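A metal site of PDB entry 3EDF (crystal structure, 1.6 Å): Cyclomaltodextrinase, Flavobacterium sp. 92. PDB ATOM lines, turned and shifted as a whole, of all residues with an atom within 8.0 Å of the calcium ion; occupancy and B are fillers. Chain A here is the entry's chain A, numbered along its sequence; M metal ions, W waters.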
ATOM      1  N   LEU A 221     -10.977  21.605  26.006  1.00  0.00           N
ATOM      2  CA  LEU A 221     -12.102  20.668  25.852  1.00  0.00           C
ATOM      3  C   LEU A 221     -12.260  20.214  24.399  1.00  0.00           C
ATOM      4  O   LEU A 221     -12.692  19.076  24.132  1.00  0.00           O
ATOM      5  CB  LEU A 221     -13.413  21.327  26.303  1.00  0.00           C
ATOM      6  CG  LEU A 221     -13.447  21.875  27.743  1.00  0.00           C
ATOM      7  CD1 LEU A 221     -14.765  22.631  28.051  1.00  0.00           C
ATOM      8  CD2 LEU A 221     -13.159  20.752  28.764  1.00  0.00           C
ATOM      9  N   SER A 222     -11.970  21.126  23.459  1.00  0.00           N
ATOM     10  CA  SER A 222     -12.229  20.871  22.041  1.00  0.00           C
ATOM     11  C   SER A 222     -11.296  19.845  21.373  1.00  0.00           C
ATOM     12  O   SER A 222     -11.711  19.134  20.447  1.00  0.00           O
ATOM     13  CB  SER A 222     -12.225  22.209  21.285  1.00  0.00           C
ATOM     14  OG  SER A 222     -12.401  22.039  19.905  1.00  0.00           O
ATOM     15  N   HIS A 223     -10.046  19.842  21.797  1.00  0.00           N
ATOM     16  CA  HIS A 223      -9.018  19.061  21.111  1.00  0.00           C
ATOM     17  C   HIS A 223      -7.986  18.431  22.013  1.00  0.00           C
ATOM     18  O   HIS A 223      -7.841  18.774  23.207  1.00  0.00           O
ATOM     19  CB  HIS A 223      -8.296  19.940  20.043  1.00  0.00           C
ATOM     20  CG  HIS A 223      -7.615  21.155  20.612  1.00  0.00           C
ATOM     21  ND1 HIS A 223      -8.235  22.383  20.680  1.00  0.00           N
ATOM     22  CD2 HIS A 223      -6.402  21.322  21.192  1.00  0.00           C
ATOM     23  CE1 HIS A 223      -7.413  23.266  21.226  1.00  0.00           C
ATOM     24  NE2 HIS A 223      -6.293  22.638  21.550  1.00  0.00           N
ATOM     25  N   ASN A 241     -13.702  13.908  15.557  1.00  0.00           N
ATOM     26  CA  ASN A 241     -14.443  14.436  14.428  1.00  0.00           C
ATOM     27  C   ASN A 241     -13.796  14.121  13.067  1.00  0.00           C
ATOM     28  O   ASN A 241     -12.566  14.001  12.975  1.00  0.00           O
ATOM     29  CB  ASN A 241     -14.642  15.952  14.609  1.00  0.00           C
ATOM     30  CG  ASN A 241     -15.730  16.269  15.626  1.00  0.00           C
ATOM     31  OD1 ASN A 241     -15.562  17.131  16.513  1.00  0.00           O
ATOM     32  ND2 ASN A 241     -16.846  15.559  15.528  1.00  0.00           N
ATOM     33  N   THR A 249     -10.494  23.565  10.702  1.00  0.00           N
ATOM     34  CA  THR A 249     -11.462  24.640  10.909  1.00  0.00           C
ATOM     35  C   THR A 249     -10.985  25.889  10.169  1.00  0.00           C
ATOM     36  O   THR A 249      -9.756  26.170  10.075  1.00  0.00           O
ATOM     37  CB  THR A 249     -11.664  24.990  12.414  1.00  0.00           C
ATOM     38  OG1 THR A 249     -12.785  25.884  12.508  1.00  0.00           O
ATOM     39  CG2 THR A 249     -10.434  25.691  13.048  1.00  0.00           C
ATOM     40  N   GLU A 267     -20.740  23.722  11.921  1.00  0.00           N
ATOM     41  CA  GLU A 267     -20.080  22.431  12.077  1.00  0.00           C
ATOM     42  C   GLU A 267     -18.577  22.557  11.890  1.00  0.00           C
ATOM     43  O   GLU A 267     -17.796  21.951  12.624  1.00  0.00           O
ATOM     44  CB  GLU A 267     -20.675  21.433  11.073  1.00  0.00           C
ATOM     45  CG  GLU A 267     -22.109  21.114  11.369  1.00  0.00           C
ATOM     46  CD  GLU A 267     -22.256  20.329  12.644  1.00  0.00           C
ATOM     47  OE1 GLU A 267     -22.875  20.852  13.585  1.00  0.00           O
ATOM     48  OE2 GLU A 267     -21.680  19.225  12.723  1.00  0.00           O
ATOM     49  N   ASN A 268     -18.172  23.382  10.931  1.00  0.00           N
ATOM     50  CA  ASN A 268     -16.754  23.578  10.723  1.00  0.00           C
ATOM     51  C   ASN A 268     -16.100  24.230  11.934  1.00  0.00           C
ATOM     52  O   ASN A 268     -14.960  23.954  12.234  1.00  0.00           O
ATOM     53  CB  ASN A 268     -16.464  24.366   9.433  1.00  0.00           C
ATOM     54  CG  ASN A 268     -14.981  24.611   9.234  1.00  0.00           C
ATOM     55  OD1 ASN A 268     -14.469  25.662   9.591  1.00  0.00           O
ATOM     56  ND2 ASN A 268     -14.281  23.628   8.666  1.00  0.00           N
ATOM     57  N   PHE A 269     -16.834  25.094  12.615  1.00  0.00           N
ATOM     58  CA  PHE A 269     -16.250  25.738  13.780  1.00  0.00           C
ATOM     59  C   PHE A 269     -16.087  24.777  14.959  1.00  0.00           C
ATOM     60  O   PHE A 269     -15.063  24.831  15.648  1.00  0.00           O
ATOM     61  CB  PHE A 269     -17.069  26.942  14.224  1.00  0.00           C
ATOM     62  CG  PHE A 269     -16.320  27.824  15.211  1.00  0.00           C
ATOM     63  CD1 PHE A 269     -15.139  28.472  14.797  1.00  0.00           C
ATOM     64  CD2 PHE A 269     -16.797  27.988  16.516  1.00  0.00           C
ATOM     65  CE1 PHE A 269     -14.416  29.269  15.689  1.00  0.00           C
ATOM     66  CE2 PHE A 269     -16.061  28.787  17.400  1.00  0.00           C
ATOM     67  CZ  PHE A 269     -14.894  29.417  16.987  1.00  0.00           C
ATOM     68  N   THR A 270     -17.109  23.950  15.221  1.00  0.00           N
ATOM     69  CA  THR A 270     -17.088  23.108  16.411  1.00  0.00           C
ATOM     70  C   THR A 270     -16.444  21.724  16.200  1.00  0.00           C
ATOM     71  O   THR A 270     -16.105  21.052  17.168  1.00  0.00           O
ATOM     72  CB  THR A 270     -18.516  22.918  17.013  1.00  0.00           C
ATOM     73  OG1 THR A 270     -19.335  22.154  16.086  1.00  0.00           O
ATOM     74  CG2 THR A 270     -19.208  24.273  17.314  1.00  0.00           C
ATOM     75  N   LYS A 271     -16.348  21.295  14.935  1.00  0.00           N
ATOM     76  CA  LYS A 271     -15.777  19.984  14.575  1.00  0.00           C
ATOM     77  C   LYS A 271     -14.470  20.072  13.814  1.00  0.00           C
ATOM     78  O   LYS A 271     -13.661  19.125  13.853  1.00  0.00           O
ATOM     79  CB  LYS A 271     -16.779  19.157  13.755  1.00  0.00           C
ATOM     80  CG  LYS A 271     -18.007  18.735  14.525  1.00  0.00           C
ATOM     81  CD  LYS A 271     -18.868  17.742  13.721  1.00  0.00           C
ATOM     82  CE  LYS A 271     -19.888  16.990  14.604  1.00  0.00           C
ATOM     83  NZ  LYS A 271     -20.965  17.891  15.113  1.00  0.00           N
ATOM     84  N   GLY A 272     -14.255  21.179  13.098  1.00  0.00           N
ATOM     85  CA  GLY A 272     -12.984  21.410  12.391  1.00  0.00           C
ATOM     86  C   GLY A 272     -11.766  21.318  13.308  1.00  0.00           C
ATOM     87  O   GLY A 272     -11.770  21.788  14.462  1.00  0.00           O
ATOM     88  N   TRP A 273     -10.701  20.706  12.828  1.00  0.00           N
ATOM     89  CA  TRP A 273      -9.475  20.631  13.599  1.00  0.00           C
ATOM     90  C   TRP A 273      -8.739  21.955  13.666  1.00  0.00           C
ATOM     91  O   TRP A 273      -8.542  22.663  12.677  1.00  0.00           O
ATOM     92  CB  TRP A 273      -8.537  19.566  13.023  1.00  0.00           C
ATOM     93  CG  TRP A 273      -9.000  18.148  13.109  1.00  0.00           C
ATOM     94  CD1 TRP A 273     -10.283  17.664  13.067  1.00  0.00           C
ATOM     95  CD2 TRP A 273      -8.129  17.028  13.180  1.00  0.00           C
ATOM     96  NE1 TRP A 273     -10.253  16.290  13.146  1.00  0.00           N
ATOM     97  CE2 TRP A 273      -8.933  15.882  13.221  1.00  0.00           C
ATOM     98  CE3 TRP A 273      -6.722  16.897  13.235  1.00  0.00           C
ATOM     99  CZ2 TRP A 273      -8.390  14.582  13.280  1.00  0.00           C
ATOM    100  CZ3 TRP A 273      -6.164  15.605  13.320  1.00  0.00           C
ATOM    101  CH2 TRP A 273      -7.015  14.469  13.330  1.00  0.00           C
ATOM    102  N   PHE A 274      -8.274  22.291  14.870  1.00  0.00           N
ATOM    103  CA  PHE A 274      -7.585  23.555  15.061  1.00  0.00           C
ATOM    104  C   PHE A 274      -6.333  23.659  14.164  1.00  0.00           C
ATOM    105  O   PHE A 274      -6.102  24.690  13.476  1.00  0.00           O
ATOM    106  CB  PHE A 274      -7.210  23.736  16.534  1.00  0.00           C
ATOM    107  CG  PHE A 274      -6.954  25.160  16.891  1.00  0.00           C
ATOM    108  CD1 PHE A 274      -5.646  25.690  16.850  1.00  0.00           C
ATOM    109  CD2 PHE A 274      -8.007  26.014  17.179  1.00  0.00           C
ATOM    110  CE1 PHE A 274      -5.389  27.035  17.143  1.00  0.00           C
ATOM    111  CE2 PHE A 274      -7.782  27.349  17.485  1.00  0.00           C
ATOM    112  CZ  PHE A 274      -6.498  27.879  17.446  1.00  0.00           C
ATOM    113  N   MET A 278      -3.718  18.692  16.162  1.00  0.00           N
ATOM    114  CA  MET A 278      -4.708  18.772  17.267  1.00  0.00           C
ATOM    115  C   MET A 278      -6.051  18.131  16.918  1.00  0.00           C
ATOM    116  O   MET A 278      -7.027  18.820  16.573  1.00  0.00           O
ATOM    117  CB  MET A 278      -4.919  20.220  17.719  1.00  0.00           C
ATOM    118  CG  MET A 278      -3.741  20.803  18.436  1.00  0.00           C
ATOM    119  SD  MET A 278      -4.056  22.550  18.758  1.00  0.00           S
ATOM    120  CE  MET A 278      -2.682  22.850  19.868  1.00  0.00           C
ATOM    121  N   PRO A 279      -6.109  16.779  16.957  1.00  0.00           N
ATOM    122  CA  PRO A 279      -7.391  16.082  16.704  1.00  0.00           C
ATOM    123  C   PRO A 279      -8.563  16.630  17.507  1.00  0.00           C
ATOM    124  O   PRO A 279      -8.432  16.891  18.720  1.00  0.00           O
ATOM    125  CB  PRO A 279      -7.099  14.630  17.127  1.00  0.00           C
ATOM    126  CG  PRO A 279      -5.615  14.471  16.875  1.00  0.00           C
ATOM    127  CD  PRO A 279      -5.002  15.833  17.218  1.00  0.00           C
ATOM    128  N   ASP A 280      -9.685  16.778  16.831  1.00  0.00           N
ATOM    129  CA  ASP A 280     -10.843  17.450  17.424  1.00  0.00           C
ATOM    130  C   ASP A 280     -11.783  16.437  18.018  1.00  0.00           C
ATOM    131  O   ASP A 280     -12.186  15.460  17.357  1.00  0.00           O
ATOM    132  CB  ASP A 280     -11.537  18.295  16.370  1.00  0.00           C
ATOM    133  CG  ASP A 280     -12.419  19.343  17.006  1.00  0.00           C
ATOM    134  OD1 ASP A 280     -13.658  19.116  17.169  1.00  0.00           O
ATOM    135  OD2 ASP A 280     -11.821  20.362  17.383  1.00  0.00           O
ATOM    136  N   LEU A 281     -12.149  16.663  19.289  1.00  0.00           N
ATOM    137  CA  LEU A 281     -13.020  15.702  19.971  1.00  0.00           C
ATOM    138  C   LEU A 281     -14.474  15.836  19.597  1.00  0.00           C
ATOM    139  O   LEU A 281     -15.036  16.920  19.564  1.00  0.00           O
ATOM    140  CB  LEU A 281     -12.892  15.863  21.503  1.00  0.00           C
ATOM    141  CG  LEU A 281     -11.506  15.616  22.086  1.00  0.00           C
ATOM    142  CD1 LEU A 281     -11.539  15.754  23.610  1.00  0.00           C
ATOM    143  CD2 LEU A 281     -10.967  14.222  21.662  1.00  0.00           C
ATOM    144  N   ASN A 282     -15.113  14.701  19.297  1.00  0.00           N
ATOM    145  CA  ASN A 282     -16.536  14.734  19.010  1.00  0.00           C
ATOM    146  C   ASN A 282     -17.398  14.747  20.272  1.00  0.00           C
ATOM    147  O   ASN A 282     -17.809  13.673  20.805  1.00  0.00           O
ATOM    148  CB  ASN A 282     -16.908  13.503  18.172  1.00  0.00           C
ATOM    149  CG  ASN A 282     -18.370  13.484  17.820  1.00  0.00           C
ATOM    150  OD1 ASN A 282     -19.102  14.467  17.999  1.00  0.00           O
ATOM    151  ND2 ASN A 282     -18.832  12.319  17.306  1.00  0.00           N
ATOM    152  N   GLN A 283     -17.725  15.949  20.735  1.00  0.00           N
ATOM    153  CA  GLN A 283     -18.449  16.045  22.002  1.00  0.00           C
ATOM    154  C   GLN A 283     -19.947  15.775  21.869  1.00  0.00           C
ATOM    155  O   GLN A 283     -20.678  15.805  22.886  1.00  0.00           O
ATOM    156  CB  GLN A 283     -18.193  17.426  22.616  1.00  0.00           C
ATOM    157  CG  GLN A 283     -16.715  17.690  22.932  1.00  0.00           C
ATOM    158  CD  GLN A 283     -16.316  19.162  22.772  1.00  0.00           C
ATOM    159  OE1 GLN A 283     -16.844  19.857  21.916  1.00  0.00           O
ATOM    160  NE2 GLN A 283     -15.411  19.642  23.629  1.00  0.00           N
ATOM    161  N   THR A 312     -10.166  27.962  23.961  1.00  0.00           N
ATOM    162  CA  THR A 312     -10.877  27.775  22.663  1.00  0.00           C
ATOM    163  C   THR A 312     -12.378  27.561  22.868  1.00  0.00           C
ATOM    164  O   THR A 312     -12.943  26.517  22.456  1.00  0.00           O
ATOM    165  CB  THR A 312     -10.261  26.561  21.834  1.00  0.00           C
ATOM    166  OG1 THR A 312      -9.844  25.507  22.716  1.00  0.00           O
ATOM    167  CG2 THR A 312      -9.062  27.031  21.016  1.00  0.00           C
ATOM    168  N   TYR A 313     -12.989  28.508  23.570  1.00  0.00           N
ATOM    169  CA  TYR A 313     -14.277  28.219  24.177  1.00  0.00           C
ATOM    170  C   TYR A 313     -15.354  27.701  23.167  1.00  0.00           C
ATOM    171  O   TYR A 313     -15.924  26.610  23.357  1.00  0.00           O
ATOM    172  CB  TYR A 313     -14.788  29.413  25.007  1.00  0.00           C
ATOM    173  CG  TYR A 313     -15.946  28.960  25.869  1.00  0.00           C
ATOM    174  CD1 TYR A 313     -15.736  28.213  27.011  1.00  0.00           C
ATOM    175  CD2 TYR A 313     -17.277  29.231  25.477  1.00  0.00           C
ATOM    176  CE1 TYR A 313     -16.811  27.744  27.732  1.00  0.00           C
ATOM    177  CE2 TYR A 313     -18.372  28.784  26.238  1.00  0.00           C
ATOM    178  CZ  TYR A 313     -18.114  28.034  27.377  1.00  0.00           C
ATOM    179  OH  TYR A 313     -19.141  27.502  28.168  1.00  0.00           O
ATOM    180  N   GLY A 314     -15.612  28.498  22.125  1.00  0.00           N
ATOM    181  CA  GLY A 314     -16.728  28.150  21.226  1.00  0.00           C
ATOM    182  C   GLY A 314     -16.414  27.044  20.228  1.00  0.00           C
ATOM    183  O   GLY A 314     -17.288  26.688  19.444  1.00  0.00           O
ATOM    184  N   TYR A 315     -15.174  26.554  20.243  1.00  0.00           N
ATOM    185  CA  TYR A 315     -14.762  25.466  19.354  1.00  0.00           C
ATOM    186  C   TYR A 315     -15.264  24.120  19.848  1.00  0.00           C
ATOM    187  O   TYR A 315     -15.097  23.105  19.157  1.00  0.00           O
ATOM    188  CB  TYR A 315     -13.243  25.391  19.212  1.00  0.00           C
ATOM    189  CG  TYR A 315     -12.612  26.548  18.503  1.00  0.00           C
ATOM    190  CD1 TYR A 315     -12.288  26.463  17.139  1.00  0.00           C
ATOM    191  CD2 TYR A 315     -12.261  27.701  19.201  1.00  0.00           C
ATOM    192  CE1 TYR A 315     -11.665  27.519  16.480  1.00  0.00           C
ATOM    193  CE2 TYR A 315     -11.625  28.791  18.548  1.00  0.00           C
ATOM    194  CZ  TYR A 315     -11.322  28.682  17.183  1.00  0.00           C
ATOM    195  OH  TYR A 315     -10.673  29.697  16.513  1.00  0.00           O
ATOM    196  N   SER A 316     -15.862  24.107  21.040  1.00  0.00           N
ATOM    197  CA  SER A 316     -16.560  22.921  21.511  1.00  0.00           C
ATOM    198  C   SER A 316     -18.009  22.966  21.077  1.00  0.00           C
ATOM    199  O   SER A 316     -18.602  24.055  20.887  1.00  0.00           O
ATOM    200  CB  SER A 316     -16.439  22.796  23.040  1.00  0.00           C
ATOM    201  OG  SER A 316     -15.114  22.451  23.386  1.00  0.00           O
ATOM    202  N   ASP A 317     -18.611  21.790  20.903  1.00  0.00           N
ATOM    203  CA  ASP A 317     -20.026  21.699  20.580  1.00  0.00           C
ATOM    204  C   ASP A 317     -20.878  22.513  21.600  1.00  0.00           C
ATOM    205  O   ASP A 317     -20.676  22.372  22.819  1.00  0.00           O
ATOM    206  CB  ASP A 317     -20.458  20.229  20.605  1.00  0.00           C
ATOM    207  CG  ASP A 317     -21.916  20.074  20.218  1.00  0.00           C
ATOM    208  OD1 ASP A 317     -22.812  20.007  21.104  1.00  0.00           O
ATOM    209  OD2 ASP A 317     -22.201  20.076  19.000  1.00  0.00           O
HETATM  210 CA    CA M   1     -13.981  21.259  18.276  1.00  0.00          CA
HETATM  211  O   HOH W   1     -13.457  22.657  16.408  1.00  0.00           O
HETATM  212  O   HOH W   2     -15.061  19.664  19.786  1.00  0.00           O
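O of Tyr 315 is bound to the calcium ion, 2.3 Å away.
Water W1 is bound to the calcium ion (2.4 Å).
The calcium ion is bound by the side-chain hydroxyl (OG) of Ser 222.
O of Thr 270 binds the calcium ion (2.4 Å).
The calcium ion is bound by the side-chain carboxylate (OD1) of Asp 280, at 2.4 Å.
The calcium ion is bound by water W2 (2.4 Å).
The calcium ion is bound by the side-chain carboxylate (OD2) of Asp 280, 2.5 Å away.
Within 4 Å of the calcium ion: Ser 222, Thr 270, Asp 280 and Tyr 315.
The backbone NH of Ser 222 is in hydrogen-bond range of the side-chain hydroxyl of Ser 316 (3.4 Å).
The backbone carbonyl oxygen (O) of Ser 222 sits at hydrogen-bond distance from the backbone NH (N) of Leu 281 (2.8 Å).
The backbone carbonyl oxygen (O) of Asp 280 lies within hydrogen-bond range of the backbone NH (N) of Asn 241 (2.8 Å).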
